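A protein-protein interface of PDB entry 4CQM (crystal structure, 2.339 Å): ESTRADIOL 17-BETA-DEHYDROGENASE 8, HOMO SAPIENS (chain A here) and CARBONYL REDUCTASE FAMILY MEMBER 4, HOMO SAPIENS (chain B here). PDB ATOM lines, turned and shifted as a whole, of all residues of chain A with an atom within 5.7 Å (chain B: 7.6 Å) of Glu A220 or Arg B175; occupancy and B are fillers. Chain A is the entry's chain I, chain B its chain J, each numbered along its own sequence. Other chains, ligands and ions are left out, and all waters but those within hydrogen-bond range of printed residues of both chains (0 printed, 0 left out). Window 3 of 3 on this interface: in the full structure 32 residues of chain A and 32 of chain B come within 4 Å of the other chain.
Glu A220 touches one residue of chain B.
Met A221 touches none of the printed residues of chain B.
Of the printed residues of chain B, Pro A223 touches Ala B174 and Arg B175.
Printed residues of chain B within 4 Å of Met A224: Arg B175.
Printed residues of chain B within 4 Å of Gly A225: Arg B175.
Of the printed residues of chain A, Ala B174 touches Pro A223 (3.3 Å).
Arg B175 touches just these residues of chain A: Thr A219, Glu A220, Ile A222, Pro A223, Met A224 and Gly A225.
The nearest printed residue of chain B that does not touch Glu A220 is Lys B171 (9.7 Å).
The nearest residue of chain A that does not touch Arg B175 is Met A221 (4.7 Å).
Among the printed residues, pairs that only touch across the chains: Thr A219 with Arg B175 (3.9 Å), Glu A220 with Arg B175 (3.9 Å), Pro A223 with Ala B174 (3.3 Å), Met A224 with Arg B175 (3.9 Å) and Gly A225 with Arg B175 (3.5 Å).
The side-chain hydroxyl (OG1) of Thr A219 sits at hydrogen-bond distance from the backbone carbonyl oxygen (O) of Val A215.
O of Ile A222 sits at hydrogen-bond distance from NH2 of Arg B175.
NE of Arg B175 is in hydrogen-bond range of O of Pro A223, at 2.6 Å.
Of the 11 printed residues of chain B, 2 touch a printed residue of chain A.
Hydrophobic or aromatic side chains of chain B that line the printed part of chain A: Ala B174.
Hydrophobic or aromatic side chains of chain A that line the printed part of chain B: Pro A223.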
ATOM      1  N   VAL A 215       5.780   1.723   9.706  1.00  0.00           N
ATOM      2  CA  VAL A 215       5.147   1.797   8.394  1.00  0.00           C
ATOM      3  C   VAL A 215       4.148   0.653   8.220  1.00  0.00           C
ATOM      4  O   VAL A 215       3.057   0.846   7.681  1.00  0.00           O
ATOM      5  CB  VAL A 215       6.192   1.754   7.256  1.00  0.00           C
ATOM      6  CG1 VAL A 215       5.511   1.714   5.893  1.00  0.00           C
ATOM      7  CG2 VAL A 215       7.134   2.945   7.352  1.00  0.00           C
ATOM      8  N   ASP A 216       4.524  -0.533   8.691  1.00  0.00           N
ATOM      9  CA  ASP A 216       3.647  -1.701   8.633  1.00  0.00           C
ATOM     10  C   ASP A 216       2.352  -1.455   9.397  1.00  0.00           C
ATOM     11  O   ASP A 216       1.262  -1.739   8.900  1.00  0.00           O
ATOM     12  CB  ASP A 216       4.352  -2.938   9.195  1.00  0.00           C
ATOM     13  CG  ASP A 216       5.556  -3.346   8.372  1.00  0.00           C
ATOM     14  OD1 ASP A 216       5.597  -3.006   7.172  1.00  0.00           O
ATOM     15  OD2 ASP A 216       6.459  -4.009   8.925  1.00  0.00           O
ATOM     16  N   LYS A 217       2.485  -0.927  10.610  1.00  0.00           N
ATOM     17  CA  LYS A 217       1.337  -0.608  11.447  1.00  0.00           C
ATOM     18  C   LYS A 217       0.463   0.468  10.811  1.00  0.00           C
ATOM     19  O   LYS A 217      -0.763   0.372  10.824  1.00  0.00           O
ATOM     20  CB  LYS A 217       1.805  -0.160  12.833  1.00  0.00           C
ATOM     21  CG  LYS A 217       0.737   0.521  13.664  1.00  0.00           C
ATOM     22  CD  LYS A 217       1.221   0.762  15.082  1.00  0.00           C
ATOM     23  CE  LYS A 217       0.337   1.763  15.798  1.00  0.00           C
ATOM     24  NZ  LYS A 217       0.479   3.120  15.203  1.00  0.00           N
ATOM     25  N   ILE A 218       1.109   1.491  10.259  1.00  0.00           N
ATOM     26  CA  ILE A 218       0.417   2.563   9.551  1.00  0.00           C
ATOM     27  C   ILE A 218      -0.354   2.019   8.350  1.00  0.00           C
ATOM     28  O   ILE A 218      -1.501   2.398   8.111  1.00  0.00           O
ATOM     29  CB  ILE A 218       1.408   3.647   9.078  1.00  0.00           C
ATOM     30  CG1 ILE A 218       1.918   4.459  10.270  1.00  0.00           C
ATOM     31  CG2 ILE A 218       0.763   4.567   8.054  1.00  0.00           C
ATOM     32  CD1 ILE A 218       3.093   5.349   9.935  1.00  0.00           C
ATOM     33  N   THR A 219       0.288   1.125   7.605  1.00  0.00           N
ATOM     34  CA  THR A 219      -0.315   0.508   6.429  1.00  0.00           C
ATOM     35  C   THR A 219      -1.610  -0.219   6.781  1.00  0.00           C
ATOM     36  O   THR A 219      -2.604  -0.122   6.061  1.00  0.00           O
ATOM     37  CB  THR A 219       0.658  -0.482   5.762  1.00  0.00           C
ATOM     38  OG1 THR A 219       1.875   0.196   5.428  1.00  0.00           O
ATOM     39  CG2 THR A 219       0.050  -1.068   4.500  1.00  0.00           C
ATOM     40  N   GLU A 220      -1.596  -0.934   7.901  1.00  0.00           N
ATOM     41  CA  GLU A 220      -2.771  -1.665   8.360  1.00  0.00           C
ATOM     42  C   GLU A 220      -3.789  -0.742   9.029  1.00  0.00           C
ATOM     43  O   GLU A 220      -4.845  -1.190   9.476  1.00  0.00           O
ATOM     44  CB  GLU A 220      -2.359  -2.782   9.320  1.00  0.00           C
ATOM     45  CG  GLU A 220      -1.629  -3.932   8.643  1.00  0.00           C
ATOM     46  CD  GLU A 220      -0.957  -4.864   9.633  1.00  0.00           C
ATOM     47  OE1 GLU A 220      -0.489  -4.379  10.683  1.00  0.00           O
ATOM     48  OE2 GLU A 220      -0.898  -6.081   9.359  1.00  0.00           O
ATOM     49  N   MET A 221      -3.466   0.546   9.096  1.00  0.00           N
ATOM     50  CA  MET A 221      -4.385   1.539   9.639  1.00  0.00           C
ATOM     51  C   MET A 221      -5.047   2.334   8.520  1.00  0.00           C
ATOM     52  O   MET A 221      -6.192   2.766   8.646  1.00  0.00           O
ATOM     53  CB  MET A 221      -3.660   2.484  10.599  1.00  0.00           C
ATOM     54  CG  MET A 221      -3.373   1.883  11.964  1.00  0.00           C
ATOM     55  SD  MET A 221      -2.486   3.027  13.036  1.00  0.00           S
ATOM     56  CE  MET A 221      -3.565   4.455  12.966  1.00  0.00           C
ATOM     57  N   ILE A 222      -4.314   2.531   7.428  1.00  0.00           N
ATOM     58  CA  ILE A 222      -4.871   3.176   6.246  1.00  0.00           C
ATOM     59  C   ILE A 222      -5.942   2.278   5.637  1.00  0.00           C
ATOM     60  O   ILE A 222      -5.675   1.116   5.331  1.00  0.00           O
ATOM     61  CB  ILE A 222      -3.787   3.479   5.194  1.00  0.00           C
ATOM     62  CG1 ILE A 222      -2.673   4.333   5.802  1.00  0.00           C
ATOM     63  CG2 ILE A 222      -4.394   4.178   3.988  1.00  0.00           C
ATOM     64  CD1 ILE A 222      -1.519   4.592   4.858  1.00  0.00           C
ATOM     65  N   PRO A 223      -7.164   2.809   5.482  1.00  0.00           N
ATOM     66  CA  PRO A 223      -8.309   2.064   4.945  1.00  0.00           C
ATOM     67  C   PRO A 223      -8.027   1.396   3.600  1.00  0.00           C
ATOM     68  O   PRO A 223      -8.475   0.271   3.377  1.00  0.00           O
ATOM     69  CB  PRO A 223      -9.384   3.143   4.801  1.00  0.00           C
ATOM     70  CG  PRO A 223      -9.054   4.123   5.865  1.00  0.00           C
ATOM     71  CD  PRO A 223      -7.550   4.163   5.919  1.00  0.00           C
ATOM     72  N   MET A 224      -7.293   2.074   2.722  1.00  0.00           N
ATOM     73  CA  MET A 224      -6.940   1.499   1.428  1.00  0.00           C
ATOM     74  C   MET A 224      -5.874   0.417   1.579  1.00  0.00           C
ATOM     75  O   MET A 224      -5.688  -0.413   0.690  1.00  0.00           O
ATOM     76  CB  MET A 224      -6.457   2.585   0.465  1.00  0.00           C
ATOM     77  CG  MET A 224      -7.536   3.575   0.063  1.00  0.00           C
ATOM     78  SD  MET A 224      -7.017   4.623  -1.306  1.00  0.00           S
ATOM     79  CE  MET A 224      -8.400   5.752  -1.409  1.00  0.00           C
ATOM     80  N   GLY A 225      -5.174   0.437   2.709  1.00  0.00           N
ATOM     81  CA  GLY A 225      -4.233  -0.616   3.043  1.00  0.00           C
ATOM     82  C   GLY A 225      -2.877  -0.503   2.375  1.00  0.00           C
ATOM     83  O   GLY A 225      -2.192  -1.507   2.186  1.00  0.00           O
ATOM     84  N   GLN B 133     -14.349  -5.752  -8.509  1.00  0.00           N
ATOM     85  CA  GLN B 133     -13.234  -5.455  -7.604  1.00  0.00           C
ATOM     86  C   GLN B 133     -12.746  -4.012  -7.696  1.00  0.00           C
ATOM     87  O   GLN B 133     -11.544  -3.754  -7.662  1.00  0.00           O
ATOM     88  CB  GLN B 133     -12.058  -6.400  -7.868  1.00  0.00           C
ATOM     89  CG  GLN B 133     -12.287  -7.836  -7.427  1.00  0.00           C
ATOM     90  CD  GLN B 133     -12.971  -8.670  -8.489  1.00  0.00           C
ATOM     91  OE1 GLN B 133     -13.180  -8.215  -9.613  1.00  0.00           O
ATOM     92  NE2 GLN B 133     -13.323  -9.902  -8.138  1.00  0.00           N
ATOM     93  N   LEU B 169     -19.146   4.320   5.048  1.00  0.00           N
ATOM     94  CA  LEU B 169     -19.136   3.376   3.938  1.00  0.00           C
ATOM     95  C   LEU B 169     -17.745   3.284   3.324  1.00  0.00           C
ATOM     96  O   LEU B 169     -17.327   2.218   2.872  1.00  0.00           O
ATOM     97  CB  LEU B 169     -20.158   3.782   2.874  1.00  0.00           C
ATOM     98  CG  LEU B 169     -20.260   2.866   1.651  1.00  0.00           C
ATOM     99  CD1 LEU B 169     -20.599   1.443   2.070  1.00  0.00           C
ATOM    100  CD2 LEU B 169     -21.285   3.395   0.661  1.00  0.00           C
ATOM    101  N   ALA B 170     -17.035   4.409   3.313  1.00  0.00           N
ATOM    102  CA  ALA B 170     -15.680   4.455   2.774  1.00  0.00           C
ATOM    103  C   ALA B 170     -14.760   3.520   3.548  1.00  0.00           C
ATOM    104  O   ALA B 170     -13.999   2.759   2.955  1.00  0.00           O
ATOM    105  CB  ALA B 170     -15.142   5.875   2.804  1.00  0.00           C
ATOM    106  N   LYS B 171     -14.838   3.580   4.872  1.00  0.00           N
ATOM    107  CA  LYS B 171     -14.055   2.699   5.730  1.00  0.00           C
ATOM    108  C   LYS B 171     -14.480   1.244   5.563  1.00  0.00           C
ATOM    109  O   LYS B 171     -13.660   0.330   5.632  1.00  0.00           O
ATOM    110  CB  LYS B 171     -14.195   3.108   7.196  1.00  0.00           C
ATOM    111  CG  LYS B 171     -13.684   4.499   7.521  1.00  0.00           C
ATOM    112  CD  LYS B 171     -13.899   4.816   8.991  1.00  0.00           C
ATOM    113  CE  LYS B 171     -13.250   6.130   9.382  1.00  0.00           C
ATOM    114  NZ  LYS B 171     -13.451   6.437  10.825  1.00  0.00           N
ATOM    115  N   GLU B 172     -15.775   1.045   5.340  1.00  0.00           N
ATOM    116  CA  GLU B 172     -16.366  -0.286   5.302  1.00  0.00           C
ATOM    117  C   GLU B 172     -15.953  -1.087   4.067  1.00  0.00           C
ATOM    118  O   GLU B 172     -15.879  -2.315   4.112  1.00  0.00           O
ATOM    119  CB  GLU B 172     -17.894  -0.172   5.366  1.00  0.00           C
ATOM    120  CG  GLU B 172     -18.639  -1.497   5.360  1.00  0.00           C
ATOM    121  CD  GLU B 172     -20.137  -1.323   5.535  1.00  0.00           C
ATOM    122  OE1 GLU B 172     -20.547  -0.539   6.417  1.00  0.00           O
ATOM    123  OE2 GLU B 172     -20.904  -1.972   4.793  1.00  0.00           O
ATOM    124  N   VAL B 173     -15.667  -0.393   2.969  1.00  0.00           N
ATOM    125  CA  VAL B 173     -15.454  -1.067   1.694  1.00  0.00           C
ATOM    126  C   VAL B 173     -14.157  -0.616   1.000  1.00  0.00           C
ATOM    127  O   VAL B 173     -13.925  -0.910  -0.175  1.00  0.00           O
ATOM    128  CB  VAL B 173     -16.677  -0.840   0.763  1.00  0.00           C
ATOM    129  CG1 VAL B 173     -16.641   0.552   0.136  1.00  0.00           C
ATOM    130  CG2 VAL B 173     -16.783  -1.937  -0.293  1.00  0.00           C
ATOM    131  N   ALA B 174     -13.298   0.073   1.745  1.00  0.00           N
ATOM    132  CA  ALA B 174     -12.031   0.557   1.201  1.00  0.00           C
ATOM    133  C   ALA B 174     -11.131  -0.584   0.730  1.00  0.00           C
ATOM    134  O   ALA B 174     -10.382  -0.435  -0.236  1.00  0.00           O
ATOM    135  CB  ALA B 174     -11.301   1.402   2.232  1.00  0.00           C
ATOM    136  N   ARG B 175     -11.209  -1.722   1.413  1.00  0.00           N
ATOM    137  CA  ARG B 175     -10.369  -2.870   1.083  1.00  0.00           C
ATOM    138  C   ARG B 175     -10.840  -3.576  -0.184  1.00  0.00           C
ATOM    139  O   ARG B 175     -10.113  -4.388  -0.757  1.00  0.00           O
ATOM    140  CB  ARG B 175     -10.333  -3.856   2.253  1.00  0.00           C
ATOM    141  CG  ARG B 175      -9.563  -3.339   3.456  1.00  0.00           C
ATOM    142  CD  ARG B 175      -8.125  -3.020   3.075  1.00  0.00           C
ATOM    143  NE  ARG B 175      -7.492  -2.101   4.016  1.00  0.00           N
ATOM    144  CZ  ARG B 175      -6.725  -2.480   5.033  1.00  0.00           C
ATOM    145  NH1 ARG B 175      -6.490  -3.767   5.248  1.00  0.00           N
ATOM    146  NH2 ARG B 175      -6.192  -1.569   5.837  1.00  0.00           N
ATOM    147  N   LYS B 176     -12.056  -3.263  -0.619  1.00  0.00           N
ATOM    148  CA  LYS B 176     -12.597  -3.841  -1.843  1.00  0.00           C
ATOM    149  C   LYS B 176     -12.366  -2.910  -3.030  1.00  0.00           C
ATOM    150  O   LYS B 176     -13.073  -2.985  -4.036  1.00  0.00           O
ATOM    151  CB  LYS B 176     -14.089  -4.139  -1.686  1.00  0.00           C
ATOM    152  CG  LYS B 176     -14.423  -5.069  -0.528  1.00  0.00           C
ATOM    153  CD  LYS B 176     -13.581  -6.336  -0.563  1.00  0.00           C
ATOM    154  CE  LYS B 176     -14.116  -7.376   0.411  1.00  0.00           C
ATOM    155  NZ  LYS B 176     -14.334  -6.807   1.771  1.00  0.00           N
ATOM    156  N   LYS B 177     -11.370  -2.037  -2.893  1.00  0.00           N
ATOM    157  CA  LYS B 177     -10.996  -1.084  -3.937  1.00  0.00           C
ATOM    158  C   LYS B 177     -12.157  -0.181  -4.340  1.00  0.00           C
ATOM    159  O   LYS B 177     -12.307   0.168  -5.511  1.00  0.00           O
ATOM    160  CB  LYS B 177     -10.457  -1.811  -5.173  1.00  0.00           C
ATOM    161  CG  LYS B 177      -9.102  -2.474  -4.983  1.00  0.00           C
ATOM    162  CD  LYS B 177      -9.227  -3.876  -4.407  1.00  0.00           C
ATOM    163  CE  LYS B 177      -7.866  -4.547  -4.293  1.00  0.00           C
ATOM    164  NZ  LYS B 177      -7.956  -5.913  -3.702  1.00  0.00           N
ATOM    165  N   ILE B 178     -12.974   0.198  -3.365  1.00  0.00           N
ATOM    166  CA  ILE B 178     -14.112   1.070  -3.627  1.00  0.00           C
ATOM    167  C   ILE B 178     -13.999   2.357  -2.821  1.00  0.00           C
ATOM    168  O   ILE B 178     -13.980   2.332  -1.590  1.00  0.00           O
ATOM    169  CB  ILE B 178     -15.442   0.374  -3.300  1.00  0.00           C
ATOM    170  CG1 ILE B 178     -15.616  -0.874  -4.167  1.00  0.00           C
ATOM    171  CG2 ILE B 178     -16.606   1.330  -3.502  1.00  0.00           C
ATOM    172  CD1 ILE B 178     -16.875  -1.651  -3.871  1.00  0.00           C
